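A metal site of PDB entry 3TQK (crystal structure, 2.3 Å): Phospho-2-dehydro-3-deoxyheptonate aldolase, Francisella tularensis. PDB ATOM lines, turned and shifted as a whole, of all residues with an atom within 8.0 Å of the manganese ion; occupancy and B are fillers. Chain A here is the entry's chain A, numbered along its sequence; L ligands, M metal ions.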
ATOM      1  N   GLY A  56     -19.382 -10.300 -10.225  1.00  0.00           N
ATOM      2  CA  GLY A  56     -19.581 -11.094  -9.025  1.00  0.00           C
ATOM      3  C   GLY A  56     -18.915 -12.441  -9.145  1.00  0.00           C
ATOM      4  O   GLY A  56     -18.131 -12.663 -10.073  1.00  0.00           O
ATOM      5  N   PRO A  57     -19.192 -13.333  -8.178  1.00  0.00           N
ATOM      6  CA  PRO A  57     -18.617 -14.675  -8.141  1.00  0.00           C
ATOM      7  C   PRO A  57     -18.985 -15.513  -9.356  1.00  0.00           C
ATOM      8  O   PRO A  57     -20.048 -15.316  -9.948  1.00  0.00           O
ATOM      9  CB  PRO A  57     -19.247 -15.277  -6.889  1.00  0.00           C
ATOM     10  CG  PRO A  57     -19.573 -14.110  -6.036  1.00  0.00           C
ATOM     11  CD  PRO A  57     -19.991 -13.047  -6.976  1.00  0.00           C
ATOM     12  N   CYS A  58     -18.107 -16.451  -9.724  1.00  0.00           N
ATOM     13  CA  CYS A  58     -18.391 -17.368 -10.831  1.00  0.00           C
ATOM     14  C   CYS A  58     -19.746 -18.019 -10.595  1.00  0.00           C
ATOM     15  O   CYS A  58     -20.633 -17.969 -11.455  1.00  0.00           O
ATOM     16  CB  CYS A  58     -17.294 -18.438 -10.976  1.00  0.00           C
ATOM     17  SG  CYS A  58     -17.719 -19.761 -12.170  1.00  0.00           S
ATOM     18  N   SER A  59     -19.905 -18.609  -9.408  1.00  0.00           N
ATOM     19  CA  SER A  59     -21.168 -19.231  -8.997  1.00  0.00           C
ATOM     20  C   SER A  59     -21.298 -19.106  -7.479  1.00  0.00           C
ATOM     21  O   SER A  59     -20.290 -19.094  -6.772  1.00  0.00           O
ATOM     22  CB  SER A  59     -21.147 -20.710  -9.368  1.00  0.00           C
ATOM     23  OG  SER A  59     -20.118 -21.376  -8.641  1.00  0.00           O
ATOM     24  N   ARG A  89     -23.629 -10.272 -10.067  1.00  0.00           N
ATOM     25  CA  ARG A  89     -23.720 -11.582 -10.652  1.00  0.00           C
ATOM     26  C   ARG A  89     -24.076 -12.593  -9.568  1.00  0.00           C
ATOM     27  O   ARG A  89     -23.332 -12.790  -8.606  1.00  0.00           O
ATOM     28  CB  ARG A  89     -22.354 -11.897 -11.277  1.00  0.00           C
ATOM     29  CG  ARG A  89     -22.244 -13.179 -12.039  1.00  0.00           C
ATOM     30  CD  ARG A  89     -20.766 -13.505 -12.292  1.00  0.00           C
ATOM     31  NE  ARG A  89     -20.676 -14.924 -12.626  1.00  0.00           N
ATOM     32  CZ  ARG A  89     -20.804 -15.420 -13.850  1.00  0.00           C
ATOM     33  NH1 ARG A  89     -20.953 -14.624 -14.891  1.00  0.00           N
ATOM     34  NH2 ARG A  89     -20.741 -16.738 -14.024  1.00  0.00           N
ATOM     35  N   TYR A  91     -25.061 -16.281  -9.796  1.00  0.00           N
ATOM     36  CA  TYR A  91     -25.235 -17.479 -10.625  1.00  0.00           C
ATOM     37  C   TYR A  91     -25.373 -18.734  -9.789  1.00  0.00           C
ATOM     38  O   TYR A  91     -24.651 -18.921  -8.808  1.00  0.00           O
ATOM     39  CB  TYR A  91     -24.096 -17.624 -11.610  1.00  0.00           C
ATOM     40  CG  TYR A  91     -24.302 -16.819 -12.874  1.00  0.00           C
ATOM     41  CD1 TYR A  91     -24.664 -15.475 -12.822  1.00  0.00           C
ATOM     42  CD2 TYR A  91     -24.143 -17.404 -14.123  1.00  0.00           C
ATOM     43  CE1 TYR A  91     -24.852 -14.736 -13.971  1.00  0.00           C
ATOM     44  CE2 TYR A  91     -24.330 -16.650 -15.289  1.00  0.00           C
ATOM     45  CZ  TYR A  91     -24.682 -15.316 -15.199  1.00  0.00           C
ATOM     46  OH  TYR A  91     -24.867 -14.553 -16.345  1.00  0.00           O
ATOM     47  N   GLU A  93     -25.500 -22.065 -11.096  1.00  0.00           N
ATOM     48  CA  GLU A  93     -25.212 -23.265 -11.873  1.00  0.00           C
ATOM     49  C   GLU A  93     -23.842 -23.148 -12.543  1.00  0.00           C
ATOM     50  O   GLU A  93     -23.450 -22.082 -13.028  1.00  0.00           O
ATOM     51  CB  GLU A  93     -26.327 -23.487 -12.910  1.00  0.00           C
ATOM     52  CG  GLU A  93     -26.436 -24.898 -13.500  1.00  0.00           C
ATOM     53  CD  GLU A  93     -25.910 -25.026 -14.942  1.00  0.00           C
ATOM     54  OE1 GLU A  93     -25.073 -24.192 -15.377  1.00  0.00           O
ATOM     55  OE2 GLU A  93     -26.342 -25.969 -15.645  1.00  0.00           O
ATOM     56  N   LYS A  94     -23.105 -24.244 -12.553  1.00  0.00           N
ATOM     57  CA  LYS A  94     -21.808 -24.326 -13.212  1.00  0.00           C
ATOM     58  C   LYS A  94     -21.874 -25.347 -14.355  1.00  0.00           C
ATOM     59  O   LYS A  94     -22.194 -26.514 -14.134  1.00  0.00           O
ATOM     60  CB  LYS A  94     -20.738 -24.733 -12.206  1.00  0.00           C
ATOM     61  CG  LYS A  94     -19.332 -24.942 -12.797  1.00  0.00           C
ATOM     62  CD  LYS A  94     -18.784 -23.699 -13.476  1.00  0.00           C
ATOM     63  CE  LYS A  94     -17.384 -23.958 -14.022  1.00  0.00           C
ATOM     64  NZ  LYS A  94     -17.438 -24.829 -15.213  1.00  0.00           N
ATOM     65  N   PRO A  95     -21.601 -24.894 -15.594  1.00  0.00           N
ATOM     66  CA  PRO A  95     -21.461 -25.854 -16.709  1.00  0.00           C
ATOM     67  C   PRO A  95     -20.342 -26.874 -16.501  1.00  0.00           C
ATOM     68  O   PRO A  95     -19.249 -26.512 -16.033  1.00  0.00           O
ATOM     69  CB  PRO A  95     -21.122 -24.959 -17.910  1.00  0.00           C
ATOM     70  CG  PRO A  95     -21.075 -23.515 -17.389  1.00  0.00           C
ATOM     71  CD  PRO A  95     -21.716 -23.503 -16.058  1.00  0.00           C
ATOM     72  N   LYS A 183     -24.981 -15.626 -24.986  1.00  0.00           N
ATOM     73  CA  LYS A 183     -23.569 -15.877 -25.208  1.00  0.00           C
ATOM     74  C   LYS A 183     -23.325 -16.503 -26.586  1.00  0.00           C
ATOM     75  O   LYS A 183     -24.151 -17.259 -27.075  1.00  0.00           O
ATOM     76  CB  LYS A 183     -23.022 -16.764 -24.089  1.00  0.00           C
ATOM     77  CG  LYS A 183     -22.971 -16.035 -22.749  1.00  0.00           C
ATOM     78  CD  LYS A 183     -22.009 -16.663 -21.753  1.00  0.00           C
ATOM     79  CE  LYS A 183     -21.215 -15.583 -21.003  1.00  0.00           C
ATOM     80  NZ  LYS A 183     -20.154 -16.175 -20.136  1.00  0.00           N
ATOM     81  N   ASP A 263     -17.667 -10.426 -22.186  1.00  0.00           N
ATOM     82  CA  ASP A 263     -17.237 -11.153 -20.991  1.00  0.00           C
ATOM     83  C   ASP A 263     -15.727 -11.035 -20.913  1.00  0.00           C
ATOM     84  O   ASP A 263     -15.047 -11.454 -21.848  1.00  0.00           O
ATOM     85  CB  ASP A 263     -17.649 -12.622 -21.118  1.00  0.00           C
ATOM     86  CG  ASP A 263     -17.522 -13.400 -19.793  1.00  0.00           C
ATOM     87  OD1 ASP A 263     -16.784 -12.942 -18.881  1.00  0.00           O
ATOM     88  OD2 ASP A 263     -18.151 -14.480 -19.678  1.00  0.00           O
ATOM     89  N   SER A 265     -14.006 -12.699 -18.826  1.00  0.00           N
ATOM     90  CA  SER A 265     -13.582 -13.981 -18.271  1.00  0.00           C
ATOM     91  C   SER A 265     -13.845 -15.137 -19.245  1.00  0.00           C
ATOM     92  O   SER A 265     -13.968 -14.926 -20.456  1.00  0.00           O
ATOM     93  CB  SER A 265     -14.327 -14.217 -16.937  1.00  0.00           C
ATOM     94  OG  SER A 265     -13.682 -15.190 -16.162  1.00  0.00           O
ATOM     95  N   HIS A 266     -13.916 -16.347 -18.707  1.00  0.00           N
ATOM     96  CA  HIS A 266     -14.150 -17.584 -19.491  1.00  0.00           C
ATOM     97  C   HIS A 266     -13.260 -17.653 -20.734  1.00  0.00           C
ATOM     98  O   HIS A 266     -12.035 -17.582 -20.605  1.00  0.00           O
ATOM     99  CB  HIS A 266     -15.646 -17.734 -19.800  1.00  0.00           C
ATOM    100  CG  HIS A 266     -16.489 -17.708 -18.566  1.00  0.00           C
ATOM    101  ND1 HIS A 266     -17.243 -16.606 -18.212  1.00  0.00           N
ATOM    102  CD2 HIS A 266     -16.648 -18.618 -17.579  1.00  0.00           C
ATOM    103  CE1 HIS A 266     -17.863 -16.857 -17.061  1.00  0.00           C
ATOM    104  NE2 HIS A 266     -17.504 -18.062 -16.655  1.00  0.00           N
ATOM    105  N   LYS A 271      -9.766 -18.590 -19.138  1.00  0.00           N
ATOM    106  CA  LYS A 271      -9.868 -19.154 -17.785  1.00  0.00           C
ATOM    107  C   LYS A 271      -8.816 -18.599 -16.786  1.00  0.00           C
ATOM    108  O   LYS A 271      -8.826 -18.964 -15.601  1.00  0.00           O
ATOM    109  CB  LYS A 271      -9.788 -20.702 -17.836  1.00  0.00           C
ATOM    110  CG  LYS A 271     -10.979 -21.420 -17.191  1.00  0.00           C
ATOM    111  CD  LYS A 271     -12.049 -21.814 -18.236  1.00  0.00           C
ATOM    112  CE  LYS A 271     -13.370 -22.270 -17.593  1.00  0.00           C
ATOM    113  NZ  LYS A 271     -14.392 -21.170 -17.542  1.00  0.00           N
ATOM    114  N   GLU A 299     -15.631 -11.725 -13.431  1.00  0.00           N
ATOM    115  CA  GLU A 299     -15.782 -12.757 -12.406  1.00  0.00           C
ATOM    116  C   GLU A 299     -14.916 -12.368 -11.211  1.00  0.00           C
ATOM    117  O   GLU A 299     -13.689 -12.296 -11.328  1.00  0.00           O
ATOM    118  CB  GLU A 299     -15.460 -14.164 -12.947  1.00  0.00           C
ATOM    119  CG  GLU A 299     -16.641 -14.791 -13.726  1.00  0.00           C
ATOM    120  CD  GLU A 299     -16.404 -16.238 -14.158  1.00  0.00           C
ATOM    121  OE1 GLU A 299     -15.311 -16.568 -14.680  1.00  0.00           O
ATOM    122  OE2 GLU A 299     -17.354 -17.042 -14.019  1.00  0.00           O
ATOM    123  N   SER A 319     -13.703 -18.705  -4.756  1.00  0.00           N
ATOM    124  CA  SER A 319     -14.499 -19.465  -5.710  1.00  0.00           C
ATOM    125  C   SER A 319     -14.239 -20.969  -5.603  1.00  0.00           C
ATOM    126  O   SER A 319     -13.099 -21.407  -5.458  1.00  0.00           O
ATOM    127  CB  SER A 319     -14.235 -19.032  -7.148  1.00  0.00           C
ATOM    128  OG  SER A 319     -15.043 -19.777  -8.048  1.00  0.00           O
ATOM    129  N   THR A 321     -15.623 -22.777  -8.090  1.00  0.00           N
ATOM    130  CA  THR A 321     -15.654 -23.099  -9.519  1.00  0.00           C
ATOM    131  C   THR A 321     -14.544 -22.310 -10.248  1.00  0.00           C
ATOM    132  O   THR A 321     -13.356 -22.520  -9.954  1.00  0.00           O
ATOM    133  CB  THR A 321     -17.072 -22.843 -10.143  1.00  0.00           C
ATOM    134  OG1 THR A 321     -17.518 -21.511  -9.836  1.00  0.00           O
ATOM    135  CG2 THR A 321     -18.082 -23.827  -9.585  1.00  0.00           C
ATOM    136  N   ASP A 322     -14.886 -21.401 -11.167  1.00  0.00           N
ATOM    137  CA  ASP A 322     -13.866 -20.715 -11.970  1.00  0.00           C
ATOM    138  C   ASP A 322     -13.086 -19.699 -11.123  1.00  0.00           C
ATOM    139  O   ASP A 322     -13.558 -19.211 -10.090  1.00  0.00           O
ATOM    140  CB  ASP A 322     -14.469 -20.002 -13.198  1.00  0.00           C
ATOM    141  CG  ASP A 322     -15.055 -20.987 -14.238  1.00  0.00           C
ATOM    142  OD1 ASP A 322     -14.553 -22.130 -14.388  1.00  0.00           O
ATOM    143  OD2 ASP A 322     -16.009 -20.587 -14.945  1.00  0.00           O
ATOM    144  N   LYS A 323     -11.878 -19.389 -11.567  1.00  0.00           N
ATOM    145  CA  LYS A 323     -11.009 -18.438 -10.888  1.00  0.00           C
ATOM    146  C   LYS A 323     -11.576 -17.020 -11.019  1.00  0.00           C
ATOM    147  O   LYS A 323     -11.957 -16.590 -12.111  1.00  0.00           O
ATOM    148  CB  LYS A 323      -9.585 -18.517 -11.445  1.00  0.00           C
ATOM    149  CG  LYS A 323      -8.870 -19.843 -11.082  1.00  0.00           C
ATOM    150  CD  LYS A 323      -7.554 -20.056 -11.845  1.00  0.00           C
ATOM    151  CE  LYS A 323      -6.857 -21.339 -11.376  1.00  0.00           C
ATOM    152  NZ  LYS A 323      -5.840 -21.862 -12.330  1.00  0.00           N
ATOM    153  N   CYS A 324     -11.660 -16.322  -9.893  1.00  0.00           N
ATOM    154  CA  CYS A 324     -12.153 -14.956  -9.841  1.00  0.00           C
ATOM    155  C   CYS A 324     -11.039 -14.012  -9.372  1.00  0.00           C
ATOM    156  O   CYS A 324     -10.146 -14.417  -8.626  1.00  0.00           O
ATOM    157  CB  CYS A 324     -13.311 -14.858  -8.856  1.00  0.00           C
ATOM    158  SG  CYS A 324     -14.766 -15.879  -9.273  1.00  0.00           S
HETATM  159  C1  LIG L   1     -20.826 -19.922 -15.233  1.00  0.00           C
HETATM  160  O1  LIG L   1     -20.819 -20.039 -13.984  1.00  0.00           O
HETATM  161  O2  LIG L   1     -19.765 -19.532 -15.769  1.00  0.00           O
HETATM  162  C2  LIG L   1     -22.059 -20.232 -16.039  1.00  0.00           C
HETATM  163 MN    MN M   1     -17.657 -18.967 -14.608  1.00  0.00          MN
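Arg 89 touches the manganese ion (NH2 to MN, 3.8 Å). Within 4 Å of the manganese ion: Cys 58, Arg 89, His 266, Glu 299 and Asp 322. The nearest printed residue that does not touch the manganese ion is Lys 271 (4.9 Å).
The side-chain carboxylate (OE2) of Glu 299 sits close to the guanidinium group (NH2) of Arg 89 (3.4 Å). The side-chain carboxylate (OE1) of Glu 299 lies within hydrogen-bond range of the side-chain hydroxyl (OG) of Ser 265, at 2.6 Å. O of His 266 is in hydrogen-bond range of N of Lys 271, at 2.9 Å. The side-chain amino group (NZ) of Lys 271 is in salt-bridge range of the side-chain carboxylate (OD1) of Asp 322 (3.3 Å). SG of Cys 324 lies within hydrogen-bond range of O of Asp 322, 3.6 Å away. The guanidinium group (NH2) of Arg 89 is in hydrogen-bond range of the backbone carbonyl oxygen (O) of Cys 58 (2.9 Å). SG of Cys 58 lies close to OG1 of Thr 321 (2.9 Å). The side-chain sulfur of Cys 324 is in hydrogen-bond range of the backbone NH of Cys 58.
The manganese ion is bound by the side-chain carboxylate (OE2) of Glu 299, a ring nitrogen (NE2) of His 266, the side-chain carboxylate (OD2) of Asp 322, an oxygen (O2) of the ligand and the side-chain sulfur (SG) of Cys 58.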
